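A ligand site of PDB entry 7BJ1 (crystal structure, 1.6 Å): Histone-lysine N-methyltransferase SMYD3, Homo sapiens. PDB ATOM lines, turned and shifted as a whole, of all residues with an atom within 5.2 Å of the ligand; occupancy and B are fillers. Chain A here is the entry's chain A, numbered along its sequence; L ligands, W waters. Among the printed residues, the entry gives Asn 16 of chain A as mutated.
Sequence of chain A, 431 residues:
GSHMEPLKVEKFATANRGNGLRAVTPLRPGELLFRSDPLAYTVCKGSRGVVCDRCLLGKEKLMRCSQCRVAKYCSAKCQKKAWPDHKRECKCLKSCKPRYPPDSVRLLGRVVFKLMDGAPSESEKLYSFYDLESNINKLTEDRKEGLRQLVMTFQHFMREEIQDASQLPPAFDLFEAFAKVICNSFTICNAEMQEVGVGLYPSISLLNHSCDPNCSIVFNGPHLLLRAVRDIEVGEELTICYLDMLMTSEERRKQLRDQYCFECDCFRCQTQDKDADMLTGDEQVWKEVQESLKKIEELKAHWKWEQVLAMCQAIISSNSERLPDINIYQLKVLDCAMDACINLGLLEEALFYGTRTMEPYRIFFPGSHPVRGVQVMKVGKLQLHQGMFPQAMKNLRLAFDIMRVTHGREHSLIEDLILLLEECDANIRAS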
ATOM      1  N   ASN A  16     -14.355   7.068  14.745  1.00  0.00           N
ATOM      2  CA  ASN A  16     -14.867   5.751  14.380  1.00  0.00           C
ATOM      3  C   ASN A  16     -15.912   5.189  15.321  1.00  0.00           C
ATOM      4  O   ASN A  16     -16.124   3.979  15.354  1.00  0.00           O
ATOM      5  CB  ASN A  16     -13.711   4.741  14.218  1.00  0.00           C
ATOM      6  CG  ASN A  16     -12.862   4.603  15.466  1.00  0.00           C
ATOM      7  OD1 ASN A  16     -13.372   4.528  16.592  1.00  0.00           O
ATOM      8  ND2 ASN A  16     -11.551   4.550  15.278  1.00  0.00           N
ATOM      9  N   ARG A  17     -16.594   6.020  16.097  1.00  0.00           N
ATOM     10  CA  ARG A  17     -17.674   5.517  16.927  1.00  0.00           C
ATOM     11  C   ARG A  17     -18.858   6.480  16.914  1.00  0.00           C
ATOM     12  O   ARG A  17     -19.529   6.671  17.926  1.00  0.00           O
ATOM     13  CB  ARG A  17     -17.195   5.252  18.350  1.00  0.00           C
ATOM     14  CG  ARG A  17     -16.389   6.371  18.969  1.00  0.00           C
ATOM     15  CD  ARG A  17     -15.459   5.763  19.998  1.00  0.00           C
ATOM     16  NE  ARG A  17     -14.516   4.871  19.337  1.00  0.00           N
ATOM     17  CZ  ARG A  17     -13.599   4.136  19.971  1.00  0.00           C
ATOM     18  NH1 ARG A  17     -12.787   3.358  19.285  1.00  0.00           N
ATOM     19  NH2 ARG A  17     -13.515   4.190  21.294  1.00  0.00           N
ATOM     20  N   GLY A  18     -19.121   7.078  15.751  1.00  0.00           N
ATOM     21  CA  GLY A  18     -20.272   7.939  15.597  1.00  0.00           C
ATOM     22  C   GLY A  18     -20.109   9.258  16.336  1.00  0.00           C
ATOM     23  O   GLY A  18     -19.006   9.793  16.495  1.00  0.00           O
ATOM     24  N   ASN A  19     -21.243   9.784  16.798  1.00  0.00           N
ATOM     25  CA  ASN A  19     -21.182  11.004  17.579  1.00  0.00           C
ATOM     26  C   ASN A  19     -20.722  10.687  19.001  1.00  0.00           C
ATOM     27  O   ASN A  19     -20.847   9.551  19.480  1.00  0.00           O
ATOM     28  CB  ASN A  19     -22.538  11.703  17.599  1.00  0.00           C
ATOM     29  CG  ASN A  19     -22.957  12.126  16.230  1.00  0.00           C
ATOM     30  OD1 ASN A  19     -22.147  12.677  15.474  1.00  0.00           O
ATOM     31  ND2 ASN A  19     -24.191  11.848  15.858  1.00  0.00           N
ATOM     32  N   GLY A  20     -20.203  11.700  19.662  1.00  0.00           N
ATOM     33  CA  GLY A  20     -19.813  11.580  21.059  1.00  0.00           C
ATOM     34  C   GLY A  20     -19.858  12.910  21.780  1.00  0.00           C
ATOM     35  O   GLY A  20     -20.286  13.918  21.198  1.00  0.00           O
ATOM     36  N   TYR A 127     -29.099  16.293  22.110  1.00  0.00           N
ATOM     37  CA  TYR A 127     -29.236  15.234  21.134  1.00  0.00           C
ATOM     38  C   TYR A 127     -30.604  14.649  21.397  1.00  0.00           C
ATOM     39  O   TYR A 127     -31.024  14.570  22.556  1.00  0.00           O
ATOM     40  CB  TYR A 127     -28.079  14.249  21.350  1.00  0.00           C
ATOM     41  CG  TYR A 127     -27.761  13.163  20.350  1.00  0.00           C
ATOM     42  CD1 TYR A 127     -27.123  13.550  19.175  1.00  0.00           C
ATOM     43  CD2 TYR A 127     -27.754  11.806  20.668  1.00  0.00           C
ATOM     44  CE1 TYR A 127     -26.679  12.635  18.244  1.00  0.00           C
ATOM     45  CE2 TYR A 127     -27.281  10.862  19.733  1.00  0.00           C
ATOM     46  CZ  TYR A 127     -26.753  11.312  18.525  1.00  0.00           C
ATOM     47  OH  TYR A 127     -26.239  10.461  17.592  1.00  0.00           O
ATOM     48  N   ASP A 131     -32.271  11.671  16.822  1.00  0.00           N
ATOM     49  CA  ASP A 131     -30.858  11.599  16.490  1.00  0.00           C
ATOM     50  C   ASP A 131     -30.222  10.259  16.875  1.00  0.00           C
ATOM     51  O   ASP A 131     -29.111   9.963  16.416  1.00  0.00           O
ATOM     52  CB  ASP A 131     -30.078  12.687  17.221  1.00  0.00           C
ATOM     53  CG  ASP A 131     -30.447  14.082  16.793  1.00  0.00           C
ATOM     54  OD1 ASP A 131     -30.742  14.285  15.603  1.00  0.00           O
ATOM     55  OD2 ASP A 131     -30.459  14.967  17.684  1.00  0.00           O
ATOM     56  N   LEU A 132     -30.880   9.503  17.751  1.00  0.00           N
ATOM     57  CA  LEU A 132     -30.230   8.359  18.402  1.00  0.00           C
ATOM     58  C   LEU A 132     -29.760   7.328  17.394  1.00  0.00           C
ATOM     59  O   LEU A 132     -30.402   7.091  16.365  1.00  0.00           O
ATOM     60  CB  LEU A 132     -31.182   7.683  19.385  1.00  0.00           C
ATOM     61  CG  LEU A 132     -31.548   8.487  20.619  1.00  0.00           C
ATOM     62  CD1 LEU A 132     -32.556   7.693  21.432  1.00  0.00           C
ATOM     63  CD2 LEU A 132     -30.288   8.806  21.434  1.00  0.00           C
ATOM     64  N   GLU A 133     -28.616   6.724  17.719  1.00  0.00           N
ATOM     65  CA  GLU A 133     -28.084   5.606  16.943  1.00  0.00           C
ATOM     66  C   GLU A 133     -29.015   4.394  17.008  1.00  0.00           C
ATOM     67  O   GLU A 133     -29.471   4.005  18.082  1.00  0.00           O
ATOM     68  CB  GLU A 133     -26.695   5.249  17.467  1.00  0.00           C
ATOM     69  CG  GLU A 133     -26.103   4.030  16.770  1.00  0.00           C
ATOM     70  CD  GLU A 133     -25.725   4.334  15.342  1.00  0.00           C
ATOM     71  OE1 GLU A 133     -24.755   5.113  15.146  1.00  0.00           O
ATOM     72  OE2 GLU A 133     -26.401   3.824  14.419  1.00  0.00           O
ATOM     73  N   ASN A 135     -28.095   1.522  14.810  1.00  0.00           N
ATOM     74  CA  ASN A 135     -27.269   0.402  14.350  1.00  0.00           C
ATOM     75  C   ASN A 135     -28.001  -0.516  13.377  1.00  0.00           C
ATOM     76  O   ASN A 135     -27.686  -1.698  13.292  1.00  0.00           O
ATOM     77  CB  ASN A 135     -26.733  -0.416  15.528  1.00  0.00           C
ATOM     78  CG  ASN A 135     -25.684   0.313  16.297  1.00  0.00           C
ATOM     79  OD1 ASN A 135     -24.722   0.815  15.719  1.00  0.00           O
ATOM     80  ND2 ASN A 135     -25.838   0.368  17.610  1.00  0.00           N
ATOM     81  N   CYS A 183     -30.143  -0.021  22.092  1.00  0.00           N
ATOM     82  CA  CYS A 183     -28.799   0.442  22.370  1.00  0.00           C
ATOM     83  C   CYS A 183     -28.744   1.821  23.034  1.00  0.00           C
ATOM     84  O   CYS A 183     -27.657   2.383  23.174  1.00  0.00           O
ATOM     85  CB  CYS A 183     -27.953   0.423  21.088  1.00  0.00           C
ATOM     86  SG  CYS A 183     -28.545   1.488  19.764  1.00  0.00           S
ATOM     87  N   ASN A 184     -29.879   2.347  23.496  1.00  0.00           N
ATOM     88  CA  ASN A 184     -29.847   3.638  24.194  1.00  0.00           C
ATOM     89  C   ASN A 184     -30.634   3.631  25.508  1.00  0.00           C
ATOM     90  O   ASN A 184     -30.816   4.694  26.100  1.00  0.00           O
ATOM     91  CB  ASN A 184     -30.360   4.762  23.279  1.00  0.00           C
ATOM     92  CG  ASN A 184     -29.427   5.006  22.086  1.00  0.00           C
ATOM     93  OD1 ASN A 184     -28.379   5.639  22.237  1.00  0.00           O
ATOM     94  ND2 ASN A 184     -29.810   4.514  20.912  1.00  0.00           N
ATOM     95  N   SER A 205     -27.119   9.912  25.971  1.00  0.00           N
ATOM     96  CA  SER A 205     -26.772   8.881  25.011  1.00  0.00           C
ATOM     97  C   SER A 205     -25.668   9.293  24.051  1.00  0.00           C
ATOM     98  O   SER A 205     -25.209   8.445  23.285  1.00  0.00           O
ATOM     99  CB  SER A 205     -27.999   8.464  24.198  1.00  0.00           C
ATOM    100  OG  SER A 205     -28.855   7.675  25.008  1.00  0.00           O
ATOM    101  N   LEU A 206     -25.212  10.556  24.063  1.00  0.00           N
ATOM    102  CA  LEU A 206     -24.015  10.887  23.286  1.00  0.00           C
ATOM    103  C   LEU A 206     -22.760  10.226  23.829  1.00  0.00           C
ATOM    104  O   LEU A 206     -21.785  10.091  23.086  1.00  0.00           O
ATOM    105  CB  LEU A 206     -23.792  12.397  23.232  1.00  0.00           C
ATOM    106  CG  LEU A 206     -24.593  13.114  22.143  1.00  0.00           C
ATOM    107  CD1 LEU A 206     -24.530  14.621  22.340  1.00  0.00           C
ATOM    108  CD2 LEU A 206     -24.047  12.716  20.778  1.00  0.00           C
ATOM    109  N   LEU A 207     -22.742   9.811  25.100  1.00  0.00           N
ATOM    110  CA  LEU A 207     -21.514   9.262  25.669  1.00  0.00           C
ATOM    111  C   LEU A 207     -21.219   7.874  25.105  1.00  0.00           C
ATOM    112  O   LEU A 207     -22.041   6.962  25.220  1.00  0.00           O
ATOM    113  CB  LEU A 207     -21.609   9.217  27.195  1.00  0.00           C
ATOM    114  CG  LEU A 207     -21.679  10.585  27.898  1.00  0.00           C
ATOM    115  CD1 LEU A 207     -22.493  10.454  29.178  1.00  0.00           C
ATOM    116  CD2 LEU A 207     -20.301  11.075  28.238  1.00  0.00           C
ATOM    117  N   ASN A 208     -20.034   7.710  24.524  1.00  0.00           N
ATOM    118  CA  ASN A 208     -19.572   6.396  24.162  1.00  0.00           C
ATOM    119  C   ASN A 208     -19.029   5.622  25.375  1.00  0.00           C
ATOM    120  O   ASN A 208     -18.810   6.160  26.457  1.00  0.00           O
ATOM    121  CB  ASN A 208     -18.526   6.512  23.059  1.00  0.00           C
ATOM    122  CG  ASN A 208     -19.176   6.913  21.753  1.00  0.00           C
ATOM    123  OD1 ASN A 208     -20.173   6.321  21.370  1.00  0.00           O
ATOM    124  ND2 ASN A 208     -18.620   7.915  21.080  1.00  0.00           N
ATOM    125  N   HIS A 209     -18.813   4.333  25.158  1.00  0.00           N
ATOM    126  CA  HIS A 209     -18.441   3.375  26.189  1.00  0.00           C
ATOM    127  C   HIS A 209     -16.927   3.272  26.364  1.00  0.00           C
ATOM    128  O   HIS A 209     -16.179   3.298  25.386  1.00  0.00           O
ATOM    129  CB  HIS A 209     -18.947   1.986  25.800  1.00  0.00           C
ATOM    130  CG  HIS A 209     -18.350   0.887  26.632  1.00  0.00           C
ATOM    131  ND1 HIS A 209     -18.783   0.587  27.908  1.00  0.00           N
ATOM    132  CD2 HIS A 209     -17.296   0.067  26.391  1.00  0.00           C
ATOM    133  CE1 HIS A 209     -18.061  -0.410  28.384  1.00  0.00           C
ATOM    134  NE2 HIS A 209     -17.149  -0.743  27.478  1.00  0.00           N
ATOM    135  N   SER A 210     -16.499   3.079  27.606  1.00  0.00           N
ATOM    136  CA  SER A 210     -15.149   2.589  27.895  1.00  0.00           C
ATOM    137  C   SER A 210     -15.209   1.618  29.053  1.00  0.00           C
ATOM    138  O   SER A 210     -15.957   1.829  29.997  1.00  0.00           O
ATOM    139  CB  SER A 210     -14.198   3.738  28.242  1.00  0.00           C
ATOM    140  OG  SER A 210     -12.961   3.221  28.713  1.00  0.00           O
ATOM    141  N   TYR A 242     -20.771   1.248  30.043  1.00  0.00           N
ATOM    142  CA  TYR A 242     -22.133   0.774  29.873  1.00  0.00           C
ATOM    143  C   TYR A 242     -22.470  -0.435  30.734  1.00  0.00           C
ATOM    144  O   TYR A 242     -23.651  -0.783  30.882  1.00  0.00           O
ATOM    145  CB  TYR A 242     -22.366   0.390  28.409  1.00  0.00           C
ATOM    146  CG  TYR A 242     -22.341   1.493  27.379  1.00  0.00           C
ATOM    147  CD1 TYR A 242     -22.170   2.827  27.734  1.00  0.00           C
ATOM    148  CD2 TYR A 242     -22.522   1.191  26.019  1.00  0.00           C
ATOM    149  CE1 TYR A 242     -22.158   3.835  26.778  1.00  0.00           C
ATOM    150  CE2 TYR A 242     -22.512   2.178  25.056  1.00  0.00           C
ATOM    151  CZ  TYR A 242     -22.333   3.496  25.441  1.00  0.00           C
ATOM    152  OH  TYR A 242     -22.315   4.482  24.466  1.00  0.00           O
ATOM    153  N   TYR A 260     -25.107  -3.529  21.631  1.00  0.00           N
ATOM    154  CA  TYR A 260     -24.618  -2.241  21.140  1.00  0.00           C
ATOM    155  C   TYR A 260     -23.906  -2.340  19.802  1.00  0.00           C
ATOM    156  O   TYR A 260     -23.439  -1.316  19.290  1.00  0.00           O
ATOM    157  CB  TYR A 260     -23.656  -1.592  22.162  1.00  0.00           C
ATOM    158  CG  TYR A 260     -24.317  -1.281  23.508  1.00  0.00           C
ATOM    159  CD1 TYR A 260     -25.138  -0.158  23.668  1.00  0.00           C
ATOM    160  CD2 TYR A 260     -24.128  -2.119  24.599  1.00  0.00           C
ATOM    161  CE1 TYR A 260     -25.723   0.139  24.939  1.00  0.00           C
ATOM    162  CE2 TYR A 260     -24.732  -1.845  25.834  1.00  0.00           C
ATOM    163  CZ  TYR A 260     -25.513  -0.723  25.986  1.00  0.00           C
ATOM    164  OH  TYR A 260     -26.076  -0.469  27.214  1.00  0.00           O
ATOM    165  N   CYS A 261     -23.800  -3.534  19.229  1.00  0.00           N
ATOM    166  CA  CYS A 261     -23.163  -3.753  17.919  1.00  0.00           C
ATOM    167  C   CYS A 261     -21.802  -3.077  17.772  1.00  0.00           C
ATOM    168  O   CYS A 261     -21.530  -2.416  16.763  1.00  0.00           O
ATOM    169  CB  CYS A 261     -24.082  -3.305  16.789  1.00  0.00           C
ATOM    170  SG  CYS A 261     -25.655  -4.160  16.702  1.00  0.00           S
ATOM    171  N   PHE A 262     -20.908  -3.248  18.756  1.00  0.00           N
ATOM    172  CA  PHE A 262     -19.516  -2.882  18.499  1.00  0.00           C
ATOM    173  C   PHE A 262     -18.548  -3.808  19.213  1.00  0.00           C
ATOM    174  O   PHE A 262     -18.922  -4.562  20.119  1.00  0.00           O
ATOM    175  CB  PHE A 262     -19.201  -1.411  18.860  1.00  0.00           C
ATOM    176  CG  PHE A 262     -19.137  -1.123  20.340  1.00  0.00           C
ATOM    177  CD1 PHE A 262     -20.288  -0.806  21.042  1.00  0.00           C
ATOM    178  CD2 PHE A 262     -17.923  -1.130  21.022  1.00  0.00           C
ATOM    179  CE1 PHE A 262     -20.250  -0.520  22.404  1.00  0.00           C
ATOM    180  CE2 PHE A 262     -17.858  -0.860  22.410  1.00  0.00           C
ATOM    181  CZ  PHE A 262     -19.024  -0.556  23.087  1.00  0.00           C
ATOM    182  N   GLU A 263     -17.292  -3.770  18.730  1.00  0.00           N
ATOM    183  CA  GLU A 263     -16.169  -4.515  19.279  1.00  0.00           C
ATOM    184  C   GLU A 263     -15.317  -3.511  20.053  1.00  0.00           C
ATOM    185  O   GLU A 263     -14.976  -2.462  19.525  1.00  0.00           O
ATOM    186  CB  GLU A 263     -15.354  -5.144  18.146  1.00  0.00           C
ATOM    187  CG  GLU A 263     -16.237  -5.652  16.980  1.00  0.00           C
ATOM    188  CD  GLU A 263     -17.043  -6.894  17.330  1.00  0.00           C
ATOM    189  OE1 GLU A 263     -16.826  -7.439  18.426  1.00  0.00           O
ATOM    190  OE2 GLU A 263     -17.923  -7.310  16.514  1.00  0.00           O
ATOM    191  N   CYS A 264     -15.028  -3.818  21.306  1.00  0.00           N
ATOM    192  CA  CYS A 264     -14.305  -2.863  22.144  1.00  0.00           C
ATOM    193  C   CYS A 264     -12.817  -3.030  21.960  1.00  0.00           C
ATOM    194  O   CYS A 264     -12.288  -4.134  22.108  1.00  0.00           O
ATOM    195  CB  CYS A 264     -14.678  -3.013  23.607  1.00  0.00           C
ATOM    196  SG  CYS A 264     -13.943  -1.643  24.576  1.00  0.00           S
HETATM  197  N1  LIG L   1     -21.920   6.951  19.138  1.00  0.00           N
HETATM  198  C1  LIG L   1     -23.333   7.042  19.560  1.00  0.00           C
HETATM  199  C2  LIG L   1     -24.107   7.944  18.611  1.00  0.00           C
HETATM  200  O1  LIG L   1     -25.280   8.297  18.842  1.00  0.00           O
HETATM  201  O2  LIG L   1     -23.554   8.318  17.559  1.00  0.00           O
HETATM  202  C3  LIG L   1     -23.424   7.553  21.000  1.00  0.00           C
HETATM  203  C4  LIG L   1     -23.371   6.416  22.057  1.00  0.00           C
HETATM  204  S1  LIG L   1     -24.895   5.400  21.955  1.00  0.00           S
HETATM  205  C5  LIG L   1     -25.382   5.352  23.700  1.00  0.00           C
HETATM  206  C6  LIG L   1     -24.186   3.723  21.812  1.00  0.00           C
HETATM  207  C7  LIG L   1     -23.582   3.417  20.436  1.00  0.00           C
HETATM  208  O3  LIG L   1     -22.367   4.133  20.234  1.00  0.00           O
HETATM  209  C8  LIG L   1     -23.194   1.940  20.292  1.00  0.00           C
HETATM  210  O4  LIG L   1     -24.285   1.116  19.933  1.00  0.00           O
HETATM  211  C9  LIG L   1     -22.093   1.992  19.245  1.00  0.00           C
HETATM  212  O5  LIG L   1     -22.702   2.237  17.976  1.00  0.00           O
HETATM  213  C10 LIG L   1     -21.403   3.276  19.626  1.00  0.00           C
HETATM  214  N2  LIG L   1     -20.303   3.113  20.616  1.00  0.00           N
HETATM  215  C11 LIG L   1     -20.352   3.424  21.953  1.00  0.00           C
HETATM  216  N3  LIG L   1     -19.152   3.165  22.509  1.00  0.00           N
HETATM  217  C12 LIG L   1     -18.325   2.682  21.534  1.00  0.00           C
HETATM  218  C13 LIG L   1     -17.007   2.244  21.537  1.00  0.00           C
HETATM  219  N4  LIG L   1     -16.243   2.271  22.643  1.00  0.00           N
HETATM  220  N5  LIG L   1     -16.482   1.812  20.355  1.00  0.00           N
HETATM  221  C14 LIG L   1     -17.208   1.781  19.190  1.00  0.00           C
HETATM  222  N6  LIG L   1     -18.518   2.218  19.175  1.00  0.00           N
HETATM  223  C15 LIG L   1     -19.057   2.648  20.340  1.00  0.00           C
HETATM  224  O   HOH W   1     -24.826   8.069  15.198  1.00  0.00           O
HETATM  225  O   HOH W   2     -21.941   0.157  16.268  1.00  0.00           O
HETATM  226  O   HOH W   3     -14.126   0.212  19.888  1.00  0.00           O
HETATM  227  O   HOH W   4     -14.775   1.705  16.786  1.00  0.00           O
HETATM  228  O   HOH W   5     -19.292   1.755  16.500  1.00  0.00           O
HETATM  229  O   HOH W   6     -13.471   1.176  23.032  1.00  0.00           O
HETATM  230  O   HOH W   7     -24.476   6.855  26.717  1.00  0.00           O
HETATM  231  O   HOH W   8     -27.474   7.327  20.259  1.00  0.00           O
HETATM  232  O   HOH W   9     -22.511   5.121  16.929  1.00  0.00           O
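A sulfur (S1) of the ligand sits close to the side-chain amide oxygen of Asn 184 (3.5 Å). A sulfur (S1) of the ligand lies close to the backbone carbonyl oxygen (O) of Ser 205. A sulfur (S1) of the ligand sits close to the side-chain hydroxyl of Tyr 242 (3.7 Å). Merely in contact with the ligand: Gly 18 (3.8 Å), Glu 133 (3.6 Å), Cys 183 (3.8 Å), Leu 206 (3.7 Å), Leu 207 (3.5 Å) and Phe 262 (3.3 Å). Hydrophobic or aromatic side chains that line the ligand: Tyr 127, His 209, Tyr 242, Tyr 260 and Phe 262. Within 4 Å of the ligand: Arg 17, Gly 18, Asn 19, Tyr 127, Glu 133, Asn 135, Cys 183, Asn 184, Ser 205, Leu 206, Leu 207, Asn 208, His 209, Tyr 242, Tyr 260 and Phe 262. Along chain A the residues within 4 Å of the ligand span positions 17 to 262. The nearest printed residue that does not touch the ligand is Asn 16 (4.6 Å).
The side-chain amide nitrogen (ND2) of Asn 135 is in hydrogen-bond range of the backbone carbonyl oxygen (O) of Tyr 260 (3.4 Å). O of Asp 131 lies within hydrogen-bond range of OH of Tyr 127. The side-chain amide nitrogen (ND2) of Asn 208 is in hydrogen-bond range of the backbone carbonyl oxygen (O) of Asn 19. The side-chain sulfur of Cys 183 sits at hydrogen-bond distance from the side-chain amide nitrogen of Asn 135. A ring nitrogen (ND1) of His 209 lies within hydrogen-bond range of the backbone NH (N) of Tyr 242. The side-chain amide oxygen of Asn 184 lies close to the side-chain hydroxyl of Ser 205. The backbone carbonyl oxygen (O) of Glu 133 is in hydrogen-bond range of the side-chain amide nitrogen (ND2) of Asn 184 (2.9 Å). O of Glu 133 is in hydrogen-bond range of SG of Cys 183 (3.2 Å).
O of Tyr 260 is in hydrogen-bond range of O4 of the ligand (2.7 Å). The side-chain hydroxyl of Tyr 127 lies within hydrogen-bond range of an oxygen (O1) of the ligand (2.7 Å). O of Arg 17 sits at hydrogen-bond distance from N1 of the ligand, at 2.7 Å. The backbone NH (N) of Asn 19 lies within hydrogen-bond range of an oxygen (O2) of the ligand, 2.8 Å away. O of Asn 19 is in hydrogen-bond range of N1 of the ligand, 2.8 Å away. O4 of the ligand lies within hydrogen-bond range of ND2 of Asn 135 (2.9 Å). The side-chain amide oxygen (OD1) of Asn 208 lies within hydrogen-bond range of a nitrogen (N1) of the ligand, 2.9 Å away. The backbone NH (N) of His 209 lies within hydrogen-bond range of a nitrogen (N3) of the ligand (2.9 Å). O of His 209 is in hydrogen-bond range of N4 of the ligand (2.9 Å).
Water W1 bridges an oxygen (O2) of the ligand (2.7 Å) and the side-chain carboxylate of Glu 133 (3.0 Å). Water W8 lies within hydrogen-bond range of OD1 of Asn 184 (2.8 Å), O1 of the ligand (2.8 Å) and N of Glu 133 (2.8 Å). Water W2 lies within hydrogen-bond range of O of Cys 261, O5 of the ligand and OD1 of Asn 135. Water W3 lies within hydrogen-bond range of the backbone carbonyl oxygen of Glu 263 (2.8 Å), a nitrogen (N5) of the ligand (2.9 Å) and the guanidinium group of Arg 17 (3.5 Å). Water W9 lies within hydrogen-bond range of OE1 of Glu 133 (2.9 Å) and N1 of the ligand (2.9 Å). Water W6 bridges N4 of the ligand (3.0 Å) and NH2 of Arg 17 (3.5 Å).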
